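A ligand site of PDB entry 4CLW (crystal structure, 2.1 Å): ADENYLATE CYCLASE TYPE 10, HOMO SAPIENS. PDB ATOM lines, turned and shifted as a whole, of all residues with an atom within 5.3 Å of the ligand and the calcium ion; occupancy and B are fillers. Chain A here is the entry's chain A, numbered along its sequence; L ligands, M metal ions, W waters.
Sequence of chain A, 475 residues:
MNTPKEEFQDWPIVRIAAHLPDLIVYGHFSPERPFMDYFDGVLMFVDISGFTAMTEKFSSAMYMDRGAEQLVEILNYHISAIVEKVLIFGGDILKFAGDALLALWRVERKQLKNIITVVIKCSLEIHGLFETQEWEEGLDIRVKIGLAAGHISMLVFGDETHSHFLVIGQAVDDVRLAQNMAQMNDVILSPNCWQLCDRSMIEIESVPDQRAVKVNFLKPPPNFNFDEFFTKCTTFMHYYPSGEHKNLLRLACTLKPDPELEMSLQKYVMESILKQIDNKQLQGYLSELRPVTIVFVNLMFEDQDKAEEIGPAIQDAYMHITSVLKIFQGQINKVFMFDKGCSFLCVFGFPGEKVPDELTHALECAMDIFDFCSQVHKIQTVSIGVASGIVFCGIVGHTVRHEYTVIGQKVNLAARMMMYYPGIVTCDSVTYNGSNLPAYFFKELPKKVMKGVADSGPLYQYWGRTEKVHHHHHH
N of Gly 98 sits close to N3 of the ligand, at 3.0 Å.
Ala 97 touches the ligand.
Phe 296 touches the ligand (CZ to N5, 3.8 Å).
CZ of Phe 336 touches C10 of the ligand, 3.1 Å away.
Phe 338 touches the ligand.
CD1 of Leu 345 touches N4 of the ligand, 3.5 Å away.
Thr 405 touches the ligand (OG1 to N3, 3.6 Å).
Val 411 touches the ligand (CG1 to N2, 3.3 Å).
Ala 415 touches the ligand.
Met 419 touches the ligand (CE to O11, 3.9 Å).
Hydrophobic or aromatic side chains within 4 Å of the ligand: Ala 97, Phe 296, Phe 336, Phe 338, Leu 345, Val 411, Ala 415 and Met 419.
Within 4 Å of the ligand: Asp 47, Ile 48, Ser 49, Gly 50, Phe 51, Thr 52, Ala 97, Gly 98, Asp 99, Arg 176, Phe 296, Phe 336, Phe 338, Leu 345, Thr 405, Val 406, Val 411, Asn 412, Ala 415, Arg 416 and Met 419.
Water W3 bridges the side-chain amide oxygen (OD1) of Asn 412 (2.9 Å) and a nitrogen (N2) of the ligand (3.0 Å).
Water W1 lies within hydrogen-bond range of N of Asp 99 (3.0 Å) and N2 of the ligand (3.4 Å).
Within 4 Å of the calcium ion: Asp 47, Ile 48 and Asp 99.
The nearest printed residue that does not touch the calcium ion is Ser 49 (4.6 Å).
The backbone NH of Asp 47 lies within hydrogen-bond range of the backbone carbonyl oxygen of Lys 144 (2.8 Å).
The guanidinium group (NH1) of Arg 416 lies close to the side-chain sulfur (SD) of Met 419 (3.6 Å).
NE of Arg 416 sits at hydrogen-bond distance from O of Lys 451 (2.7 Å).
The backbone NH of Gly 98 is in hydrogen-bond range of the side-chain hydroxyl of Thr 405 (3.0 Å).
The backbone carbonyl oxygen of Leu 345 lies within hydrogen-bond range of the backbone NH of Asn 333.
Water W4 is bound to the calcium ion.
The calcium ion is bound by OD1 of Asp 99.
The calcium ion is bound by an oxygen (O1) of the ligand.
The calcium ion is bound by the side-chain carboxylate (OD1) of Asp 47, 2.4 Å away.
An oxygen (O4) of the ligand binds the calcium ion (2.5 Å).
The backbone carbonyl oxygen (O) of Ile 48 is bound to the calcium ion (2.6 Å).
The calcium ion has six donor atoms within binding distance.
The backbone NH (N) of Thr 52 sits at hydrogen-bond distance from an oxygen (O2) of the ligand, 3.0 Å away.
An oxygen (O3) of the ligand lies within hydrogen-bond range of the side-chain hydroxyl (OG1) of Thr 52 (2.6 Å).
The side-chain hydroxyl of Ser 49 sits at hydrogen-bond distance from an oxygen (O5) of the ligand.
ND2 of Asn 412 is in hydrogen-bond range of O3 of the ligand (2.8 Å).
The backbone carbonyl oxygen (O) of Val 406 is in hydrogen-bond range of a nitrogen (N3) of the ligand.
The guanidinium group of Arg 416 lies within salt-bridge range of an oxygen (O7) of the ligand (3.1 Å).
N of Gly 50 is in hydrogen-bond range of O2 of the ligand (2.9 Å).
An oxygen (O2) of the ligand is in hydrogen-bond range of the backbone NH (N) of Phe 51 (3.1 Å).
The guanidinium group of Arg 176 sits at hydrogen-bond distance from an oxygen (O12) of the ligand (3.4 Å).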
ATOM      1  N   ASP A  47      16.598 -10.957  29.131  1.00  0.00           N
ATOM      2  CA  ASP A  47      17.310 -11.484  27.943  1.00  0.00           C
ATOM      3  C   ASP A  47      18.172 -10.410  27.329  1.00  0.00           C
ATOM      4  O   ASP A  47      17.677  -9.374  26.931  1.00  0.00           O
ATOM      5  CB  ASP A  47      16.314 -12.001  26.885  1.00  0.00           C
ATOM      6  CG  ASP A  47      17.007 -12.608  25.634  1.00  0.00           C
ATOM      7  OD1 ASP A  47      18.047 -13.278  25.792  1.00  0.00           O
ATOM      8  OD2 ASP A  47      16.509 -12.397  24.483  1.00  0.00           O
ATOM      9  N   ILE A  48      19.475 -10.648  27.207  1.00  0.00           N
ATOM     10  CA  ILE A  48      20.291  -9.752  26.382  1.00  0.00           C
ATOM     11  C   ILE A  48      20.414 -10.175  24.916  1.00  0.00           C
ATOM     12  O   ILE A  48      20.714 -11.330  24.634  1.00  0.00           O
ATOM     13  CB  ILE A  48      21.708  -9.665  26.890  1.00  0.00           C
ATOM     14  CG1 ILE A  48      21.671  -9.043  28.289  1.00  0.00           C
ATOM     15  CG2 ILE A  48      22.571  -8.861  25.917  1.00  0.00           C
ATOM     16  CD1 ILE A  48      23.030  -8.993  28.932  1.00  0.00           C
ATOM     17  N   SER A  49      20.248  -9.218  24.019  1.00  0.00           N
ATOM     18  CA  SER A  49      20.458  -9.383  22.600  1.00  0.00           C
ATOM     19  C   SER A  49      21.758  -8.769  22.151  1.00  0.00           C
ATOM     20  O   SER A  49      22.190  -7.747  22.659  1.00  0.00           O
ATOM     21  CB  SER A  49      19.338  -8.696  21.793  1.00  0.00           C
ATOM     22  OG  SER A  49      18.560  -9.675  21.170  1.00  0.00           O
ATOM     23  N   GLY A  50      22.360  -9.399  21.151  1.00  0.00           N
ATOM     24  CA  GLY A  50      23.571  -8.890  20.527  1.00  0.00           C
ATOM     25  C   GLY A  50      24.804  -9.641  20.932  1.00  0.00           C
ATOM     26  O   GLY A  50      25.834  -9.461  20.331  1.00  0.00           O
ATOM     27  N   PHE A  51      24.704 -10.515  21.933  1.00  0.00           N
ATOM     28  CA  PHE A  51      25.865 -11.246  22.305  1.00  0.00           C
ATOM     29  C   PHE A  51      26.271 -12.365  21.421  1.00  0.00           C
ATOM     30  O   PHE A  51      27.488 -12.612  21.348  1.00  0.00           O
ATOM     31  CB  PHE A  51      25.873 -11.705  23.765  1.00  0.00           C
ATOM     32  CG  PHE A  51      26.569 -10.739  24.632  1.00  0.00           C
ATOM     33  CD1 PHE A  51      27.955 -10.571  24.524  1.00  0.00           C
ATOM     34  CD2 PHE A  51      25.853  -9.917  25.493  1.00  0.00           C
ATOM     35  CE1 PHE A  51      28.615  -9.613  25.294  1.00  0.00           C
ATOM     36  CE2 PHE A  51      26.503  -8.932  26.259  1.00  0.00           C
ATOM     37  CZ  PHE A  51      27.883  -8.780  26.167  1.00  0.00           C
ATOM     38  N   THR A  52      25.348 -13.062  20.752  1.00  0.00           N
ATOM     39  CA  THR A  52      25.883 -14.218  19.937  1.00  0.00           C
ATOM     40  C   THR A  52      26.545 -13.707  18.672  1.00  0.00           C
ATOM     41  O   THR A  52      27.393 -14.410  18.060  1.00  0.00           O
ATOM     42  CB  THR A  52      24.828 -15.295  19.555  1.00  0.00           C
ATOM     43  OG1 THR A  52      23.823 -14.675  18.726  1.00  0.00           O
ATOM     44  CG2 THR A  52      24.181 -15.870  20.823  1.00  0.00           C
ATOM     45  N   ALA A  53      26.125 -12.506  18.246  1.00  0.00           N
ATOM     46  CA  ALA A  53      26.804 -11.821  17.146  1.00  0.00           C
ATOM     47  C   ALA A  53      28.188 -11.349  17.593  1.00  0.00           C
ATOM     48  O   ALA A  53      29.161 -11.463  16.853  1.00  0.00           O
ATOM     49  CB  ALA A  53      25.972 -10.659  16.638  1.00  0.00           C
ATOM     50  N   ALA A  97      21.135 -18.677  31.248  1.00  0.00           N
ATOM     51  CA  ALA A  97      20.980 -19.486  30.011  1.00  0.00           C
ATOM     52  C   ALA A  97      21.583 -18.663  28.899  1.00  0.00           C
ATOM     53  O   ALA A  97      20.973 -17.725  28.372  1.00  0.00           O
ATOM     54  CB  ALA A  97      19.518 -19.791  29.770  1.00  0.00           C
ATOM     55  N   GLY A  98      22.853 -18.908  28.632  1.00  0.00           N
ATOM     56  CA  GLY A  98      23.577 -18.088  27.713  1.00  0.00           C
ATOM     57  C   GLY A  98      23.718 -16.666  28.215  1.00  0.00           C
ATOM     58  O   GLY A  98      24.306 -16.396  29.269  1.00  0.00           O
ATOM     59  N   ASP A  99      23.201 -15.737  27.427  1.00  0.00           N
ATOM     60  CA  ASP A  99      23.229 -14.309  27.774  1.00  0.00           C
ATOM     61  C   ASP A  99      21.878 -13.805  28.386  1.00  0.00           C
ATOM     62  O   ASP A  99      21.589 -12.629  28.321  1.00  0.00           O
ATOM     63  CB  ASP A  99      23.630 -13.500  26.513  1.00  0.00           C
ATOM     64  CG  ASP A  99      22.725 -13.798  25.313  1.00  0.00           C
ATOM     65  OD1 ASP A  99      21.723 -14.580  25.530  1.00  0.00           O
ATOM     66  OD2 ASP A  99      23.101 -13.342  24.161  1.00  0.00           O
ATOM     67  N   ALA A 100      21.083 -14.717  28.936  1.00  0.00           N
ATOM     68  CA  ALA A 100      19.811 -14.417  29.612  1.00  0.00           C
ATOM     69  C   ALA A 100      19.844 -15.011  31.035  1.00  0.00           C
ATOM     70  O   ALA A 100      20.572 -15.966  31.326  1.00  0.00           O
ATOM     71  CB  ALA A 100      18.662 -15.047  28.831  1.00  0.00           C
ATOM     72  N   LYS A 144      15.625  -7.256  26.810  1.00  0.00           N
ATOM     73  CA  LYS A 144      14.192  -7.466  26.912  1.00  0.00           C
ATOM     74  C   LYS A 144      13.906  -8.169  28.257  1.00  0.00           C
ATOM     75  O   LYS A 144      14.658  -9.062  28.635  1.00  0.00           O
ATOM     76  CB  LYS A 144      13.685  -8.351  25.775  1.00  0.00           C
ATOM     77  CG  LYS A 144      13.897  -7.778  24.381  1.00  0.00           C
ATOM     78  CD  LYS A 144      13.914  -8.847  23.297  1.00  0.00           C
ATOM     79  CE  LYS A 144      14.518  -8.245  22.021  1.00  0.00           C
ATOM     80  NZ  LYS A 144      14.183  -8.980  20.776  1.00  0.00           N
ATOM     81  N   ARG A 176       8.278 -16.622  29.848  1.00  0.00           N
ATOM     82  CA  ARG A 176       8.907 -16.770  28.545  1.00  0.00           C
ATOM     83  C   ARG A 176       8.061 -16.134  27.444  1.00  0.00           C
ATOM     84  O   ARG A 176       8.585 -15.447  26.614  1.00  0.00           O
ATOM     85  CB  ARG A 176       9.207 -18.234  28.174  1.00  0.00           C
ATOM     86  CG  ARG A 176      10.176 -18.328  26.979  1.00  0.00           C
ATOM     87  CD  ARG A 176      10.798 -19.731  26.801  1.00  0.00           C
ATOM     88  NE  ARG A 176      11.740 -20.042  27.869  1.00  0.00           N
ATOM     89  CZ  ARG A 176      13.073 -20.064  27.766  1.00  0.00           C
ATOM     90  NH1 ARG A 176      13.665 -19.819  26.593  1.00  0.00           N
ATOM     91  NH2 ARG A 176      13.805 -20.336  28.835  1.00  0.00           N
ATOM     92  N   PHE A 296      20.567 -30.508  21.560  1.00  0.00           N
ATOM     93  CA  PHE A 296      19.488 -29.887  22.265  1.00  0.00           C
ATOM     94  C   PHE A 296      18.268 -30.760  22.197  1.00  0.00           C
ATOM     95  O   PHE A 296      17.647 -30.973  21.103  1.00  0.00           O
ATOM     96  CB  PHE A 296      19.221 -28.506  21.645  1.00  0.00           C
ATOM     97  CG  PHE A 296      19.095 -27.397  22.634  1.00  0.00           C
ATOM     98  CD1 PHE A 296      18.348 -27.523  23.788  1.00  0.00           C
ATOM     99  CD2 PHE A 296      19.755 -26.196  22.411  1.00  0.00           C
ATOM    100  CE1 PHE A 296      18.256 -26.464  24.722  1.00  0.00           C
ATOM    101  CE2 PHE A 296      19.685 -25.134  23.318  1.00  0.00           C
ATOM    102  CZ  PHE A 296      18.933 -25.276  24.475  1.00  0.00           C
ATOM    103  N   ASN A 333      24.625 -29.515  30.011  1.00  0.00           N
ATOM    104  CA  ASN A 333      25.076 -28.206  30.440  1.00  0.00           C
ATOM    105  C   ASN A 333      23.996 -27.580  31.309  1.00  0.00           C
ATOM    106  O   ASN A 333      24.301 -26.977  32.310  1.00  0.00           O
ATOM    107  CB  ASN A 333      25.397 -27.291  29.257  1.00  0.00           C
ATOM    108  CG  ASN A 333      25.756 -25.864  29.689  1.00  0.00           C
ATOM    109  OD1 ASN A 333      24.951 -24.933  29.609  1.00  0.00           O
ATOM    110  ND2 ASN A 333      26.968 -25.691  30.142  1.00  0.00           N
ATOM    111  N   PHE A 336      16.046 -26.814  31.307  1.00  0.00           N
ATOM    112  CA  PHE A 336      15.018 -25.808  31.587  1.00  0.00           C
ATOM    113  C   PHE A 336      13.764 -26.046  30.815  1.00  0.00           C
ATOM    114  O   PHE A 336      13.767 -26.801  29.839  1.00  0.00           O
ATOM    115  CB  PHE A 336      15.520 -24.439  31.232  1.00  0.00           C
ATOM    116  CG  PHE A 336      16.255 -24.432  29.998  1.00  0.00           C
ATOM    117  CD1 PHE A 336      15.595 -24.319  28.793  1.00  0.00           C
ATOM    118  CD2 PHE A 336      17.614 -24.644  30.030  1.00  0.00           C
ATOM    119  CE1 PHE A 336      16.293 -24.359  27.597  1.00  0.00           C
ATOM    120  CE2 PHE A 336      18.319 -24.706  28.867  1.00  0.00           C
ATOM    121  CZ  PHE A 336      17.656 -24.557  27.649  1.00  0.00           C
ATOM    122  N   PHE A 338      11.101 -24.745  28.196  1.00  0.00           N
ATOM    123  CA  PHE A 338      10.781 -23.854  27.054  1.00  0.00           C
ATOM    124  C   PHE A 338       9.285 -23.645  26.965  1.00  0.00           C
ATOM    125  O   PHE A 338       8.537 -24.227  27.757  1.00  0.00           O
ATOM    126  CB  PHE A 338      11.229 -24.461  25.734  1.00  0.00           C
ATOM    127  CG  PHE A 338      12.413 -23.782  25.134  1.00  0.00           C
ATOM    128  CD1 PHE A 338      13.544 -23.503  25.888  1.00  0.00           C
ATOM    129  CD2 PHE A 338      12.418 -23.451  23.793  1.00  0.00           C
ATOM    130  CE1 PHE A 338      14.652 -22.879  25.316  1.00  0.00           C
ATOM    131  CE2 PHE A 338      13.516 -22.831  23.221  1.00  0.00           C
ATOM    132  CZ  PHE A 338      14.635 -22.549  23.980  1.00  0.00           C
ATOM    133  N   LEU A 345      20.161 -29.181  27.388  1.00  0.00           N
ATOM    134  CA  LEU A 345      21.211 -28.669  26.531  1.00  0.00           C
ATOM    135  C   LEU A 345      22.463 -29.472  26.772  1.00  0.00           C
ATOM    136  O   LEU A 345      23.078 -29.374  27.838  1.00  0.00           O
ATOM    137  CB  LEU A 345      21.441 -27.218  26.774  1.00  0.00           C
ATOM    138  CG  LEU A 345      22.271 -26.385  25.779  1.00  0.00           C
ATOM    139  CD1 LEU A 345      22.367 -24.957  26.283  1.00  0.00           C
ATOM    140  CD2 LEU A 345      23.626 -26.919  25.516  1.00  0.00           C
ATOM    141  N   THR A 405      28.385 -21.539  31.335  1.00  0.00           N
ATOM    142  CA  THR A 405      27.386 -21.515  30.255  1.00  0.00           C
ATOM    143  C   THR A 405      28.017 -21.569  28.817  1.00  0.00           C
ATOM    144  O   THR A 405      29.236 -21.462  28.656  1.00  0.00           O
ATOM    145  CB  THR A 405      26.339 -20.373  30.472  1.00  0.00           C
ATOM    146  OG1 THR A 405      25.181 -20.598  29.602  1.00  0.00           O
ATOM    147  CG2 THR A 405      26.908 -19.067  30.133  1.00  0.00           C
ATOM    148  N   VAL A 406      27.172 -21.800  27.824  1.00  0.00           N
ATOM    149  CA  VAL A 406      27.588 -21.786  26.432  1.00  0.00           C
ATOM    150  C   VAL A 406      26.750 -20.734  25.665  1.00  0.00           C
ATOM    151  O   VAL A 406      25.570 -20.574  25.903  1.00  0.00           O
ATOM    152  CB  VAL A 406      27.461 -23.143  25.786  1.00  0.00           C
ATOM    153  CG1 VAL A 406      28.457 -24.055  26.380  1.00  0.00           C
ATOM    154  CG2 VAL A 406      26.031 -23.717  25.958  1.00  0.00           C
ATOM    155  N   ILE A 407      27.419 -19.952  24.831  1.00  0.00           N
ATOM    156  CA  ILE A 407      26.792 -18.912  24.045  1.00  0.00           C
ATOM    157  C   ILE A 407      27.339 -19.056  22.639  1.00  0.00           C
ATOM    158  O   ILE A 407      28.577 -19.229  22.416  1.00  0.00           O
ATOM    159  CB  ILE A 407      27.159 -17.518  24.576  1.00  0.00           C
ATOM    160  CG1 ILE A 407      26.662 -17.362  25.979  1.00  0.00           C
ATOM    161  CG2 ILE A 407      26.588 -16.388  23.691  1.00  0.00           C
ATOM    162  CD1 ILE A 407      27.173 -16.102  26.658  1.00  0.00           C
ATOM    163  N   VAL A 411      24.437 -22.656  19.233  1.00  0.00           N
ATOM    164  CA  VAL A 411      23.578 -23.032  20.351  1.00  0.00           C
ATOM    165  C   VAL A 411      22.161 -22.583  20.002  1.00  0.00           C
ATOM    166  O   VAL A 411      21.211 -23.378  20.161  1.00  0.00           O
ATOM    167  CB  VAL A 411      24.035 -22.402  21.731  1.00  0.00           C
ATOM    168  CG1 VAL A 411      23.141 -22.851  22.819  1.00  0.00           C
ATOM    169  CG2 VAL A 411      25.487 -22.731  22.118  1.00  0.00           C
ATOM    170  N   ASN A 412      22.016 -21.335  19.535  1.00  0.00           N
ATOM    171  CA  ASN A 412      20.724 -20.831  19.085  1.00  0.00           C
ATOM    172  C   ASN A 412      20.119 -21.716  17.945  1.00  0.00           C
ATOM    173  O   ASN A 412      18.921 -22.009  17.925  1.00  0.00           O
ATOM    174  CB  ASN A 412      20.837 -19.404  18.486  1.00  0.00           C
ATOM    175  CG  ASN A 412      21.164 -18.325  19.513  1.00  0.00           C
ATOM    176  OD1 ASN A 412      21.561 -18.633  20.644  1.00  0.00           O
ATOM    177  ND2 ASN A 412      20.999 -17.064  19.121  1.00  0.00           N
ATOM    178  N   ALA A 415      18.691 -25.003  19.212  1.00  0.00           N
ATOM    179  CA  ALA A 415      17.448 -24.671  19.916  1.00  0.00           C
ATOM    180  C   ALA A 415      16.290 -24.378  18.970  1.00  0.00           C
ATOM    181  O   ALA A 415      15.210 -24.886  19.170  1.00  0.00           O
ATOM    182  CB  ALA A 415      17.629 -23.519  20.903  1.00  0.00           C
ATOM    183  N   ARG A 416      16.536 -23.612  17.899  1.00  0.00           N
ATOM    184  CA  ARG A 416      15.494 -23.337  16.939  1.00  0.00           C
ATOM    185  C   ARG A 416      15.116 -24.582  16.093  1.00  0.00           C
ATOM    186  O   ARG A 416      13.943 -24.731  15.735  1.00  0.00           O
ATOM    187  CB  ARG A 416      15.858 -22.187  15.995  1.00  0.00           C
ATOM    188  CG  ARG A 416      16.221 -20.858  16.692  1.00  0.00           C
ATOM    189  CD  ARG A 416      15.094 -20.469  17.594  1.00  0.00           C
ATOM    190  NE  ARG A 416      15.022 -19.062  17.961  1.00  0.00           N
ATOM    191  CZ  ARG A 416      14.175 -18.589  18.883  1.00  0.00           C
ATOM    192  NH1 ARG A 416      13.323 -19.400  19.528  1.00  0.00           N
ATOM    193  NH2 ARG A 416      14.166 -17.301  19.179  1.00  0.00           N
ATOM    194  N   MET A 419      12.580 -26.810  17.732  1.00  0.00           N
ATOM    195  CA  MET A 419      11.268 -26.138  17.760  1.00  0.00           C
ATOM    196  C   MET A 419      10.661 -26.103  16.377  1.00  0.00           C
ATOM    197  O   MET A 419       9.495 -26.324  16.215  1.00  0.00           O
ATOM    198  CB  MET A 419      11.359 -24.662  18.199  1.00  0.00           C
ATOM    199  CG  MET A 419      11.725 -24.432  19.658  1.00  0.00           C
ATOM    200  SD  MET A 419      11.918 -22.665  20.028  1.00  0.00           S
ATOM    201  CE  MET A 419      13.701 -22.563  20.057  1.00  0.00           C
ATOM    202  N   LYS A 451      13.635 -17.835  13.919  1.00  0.00           N
ATOM    203  CA  LYS A 451      13.845 -16.628  14.751  1.00  0.00           C
ATOM    204  C   LYS A 451      15.264 -16.461  15.228  1.00  0.00           C
ATOM    205  O   LYS A 451      15.782 -17.266  16.064  1.00  0.00           O
ATOM    206  CB  LYS A 451      12.913 -16.628  15.984  1.00  0.00           C
ATOM    207  N   GLY A 452      15.878 -15.403  14.732  1.00  0.00           N
ATOM    208  CA  GLY A 452      17.209 -15.044  15.188  1.00  0.00           C
ATOM    209  C   GLY A 452      18.198 -16.120  14.769  1.00  0.00           C
ATOM    210  O   GLY A 452      18.991 -16.641  15.591  1.00  0.00           O
HETATM  211  P1  LIG L   1      21.374 -13.354  20.898  1.00  0.00           P
HETATM  212  O1  LIG L   1      21.252 -14.062  22.240  1.00  0.00           O
HETATM  213  O2  LIG L   1      22.491 -12.306  20.752  1.00  0.00           O
HETATM  214  O3  LIG L   1      21.480 -14.433  19.860  1.00  0.00           O
HETATM  215  P2  LIG L   1      18.521 -13.055  21.051  1.00  0.00           P
HETATM  216  O4  LIG L   1      18.270 -12.872  22.491  1.00  0.00           O
HETATM  217  O5  LIG L   1      17.518 -12.003  20.345  1.00  0.00           O
HETATM  218  O6  LIG L   1      20.025 -12.483  20.737  1.00  0.00           O
HETATM  219  P3  LIG L   1      16.750 -15.632  20.982  1.00  0.00           P
HETATM  220  O7  LIG L   1      15.534 -14.792  20.389  1.00  0.00           O
HETATM  221  O8  LIG L   1      16.590 -15.839  22.456  1.00  0.00           O
HETATM  222  C1  LIG L   1      18.326 -14.795  20.527  1.00  0.00           C
HETATM  223  O9  LIG L   1      16.812 -17.105  20.301  1.00  0.00           O
HETATM  224  C2  LIG L   1      17.815 -18.012  20.737  1.00  0.00           C
HETATM  225  C3  LIG L   1      17.214 -19.274  21.311  1.00  0.00           C
HETATM  226  O10 LIG L   1      18.294 -20.122  21.683  1.00  0.00           O
HETATM  227  C4  LIG L   1      16.363 -19.077  22.563  1.00  0.00           C
HETATM  228  O11 LIG L   1      15.260 -19.965  22.445  1.00  0.00           O
HETATM  229  C5  LIG L   1      17.207 -19.557  23.722  1.00  0.00           C
HETATM  230  O12 LIG L   1      16.439 -20.225  24.730  1.00  0.00           O
HETATM  231  C6  LIG L   1      18.166 -20.551  23.046  1.00  0.00           C
HETATM  232  N1  LIG L   1      19.477 -20.575  23.736  1.00  0.00           N
HETATM  233  C7  LIG L   1      20.637 -20.092  23.253  1.00  0.00           C
HETATM  234  N2  LIG L   1      21.648 -20.254  24.137  1.00  0.00           N
HETATM  235  C8  LIG L   1      21.130 -20.881  25.204  1.00  0.00           C
HETATM  236  C9  LIG L   1      21.660 -21.352  26.514  1.00  0.00           C
HETATM  237  N3  LIG L   1      22.968 -21.236  26.820  1.00  0.00           N
HETATM  238  N4  LIG L   1      20.793 -21.966  27.347  1.00  0.00           N
HETATM  239  C10 LIG L   1      19.471 -22.127  27.038  1.00  0.00           C
HETATM  240  N5  LIG L   1      18.915 -21.718  25.877  1.00  0.00           N
HETATM  241  C11 LIG L   1      19.700 -21.101  24.941  1.00  0.00           C
HETATM  242 CA    CA M   1      19.849 -13.749  24.213  1.00  0.00          CA
HETATM  243  O   HOH W   1      22.710 -17.121  24.759  1.00  0.00           O
HETATM  244  O   HOH W   2      19.128 -18.044  26.356  1.00  0.00           O
HETATM  245  O   HOH W   3      23.708 -18.719  22.523  1.00  0.00           O
HETATM  246  O   HOH W   4      18.968 -16.004  24.242  1.00  0.00           O
HETATM  247  O   HOH W   5      21.121 -16.564  22.634  1.00  0.00           O
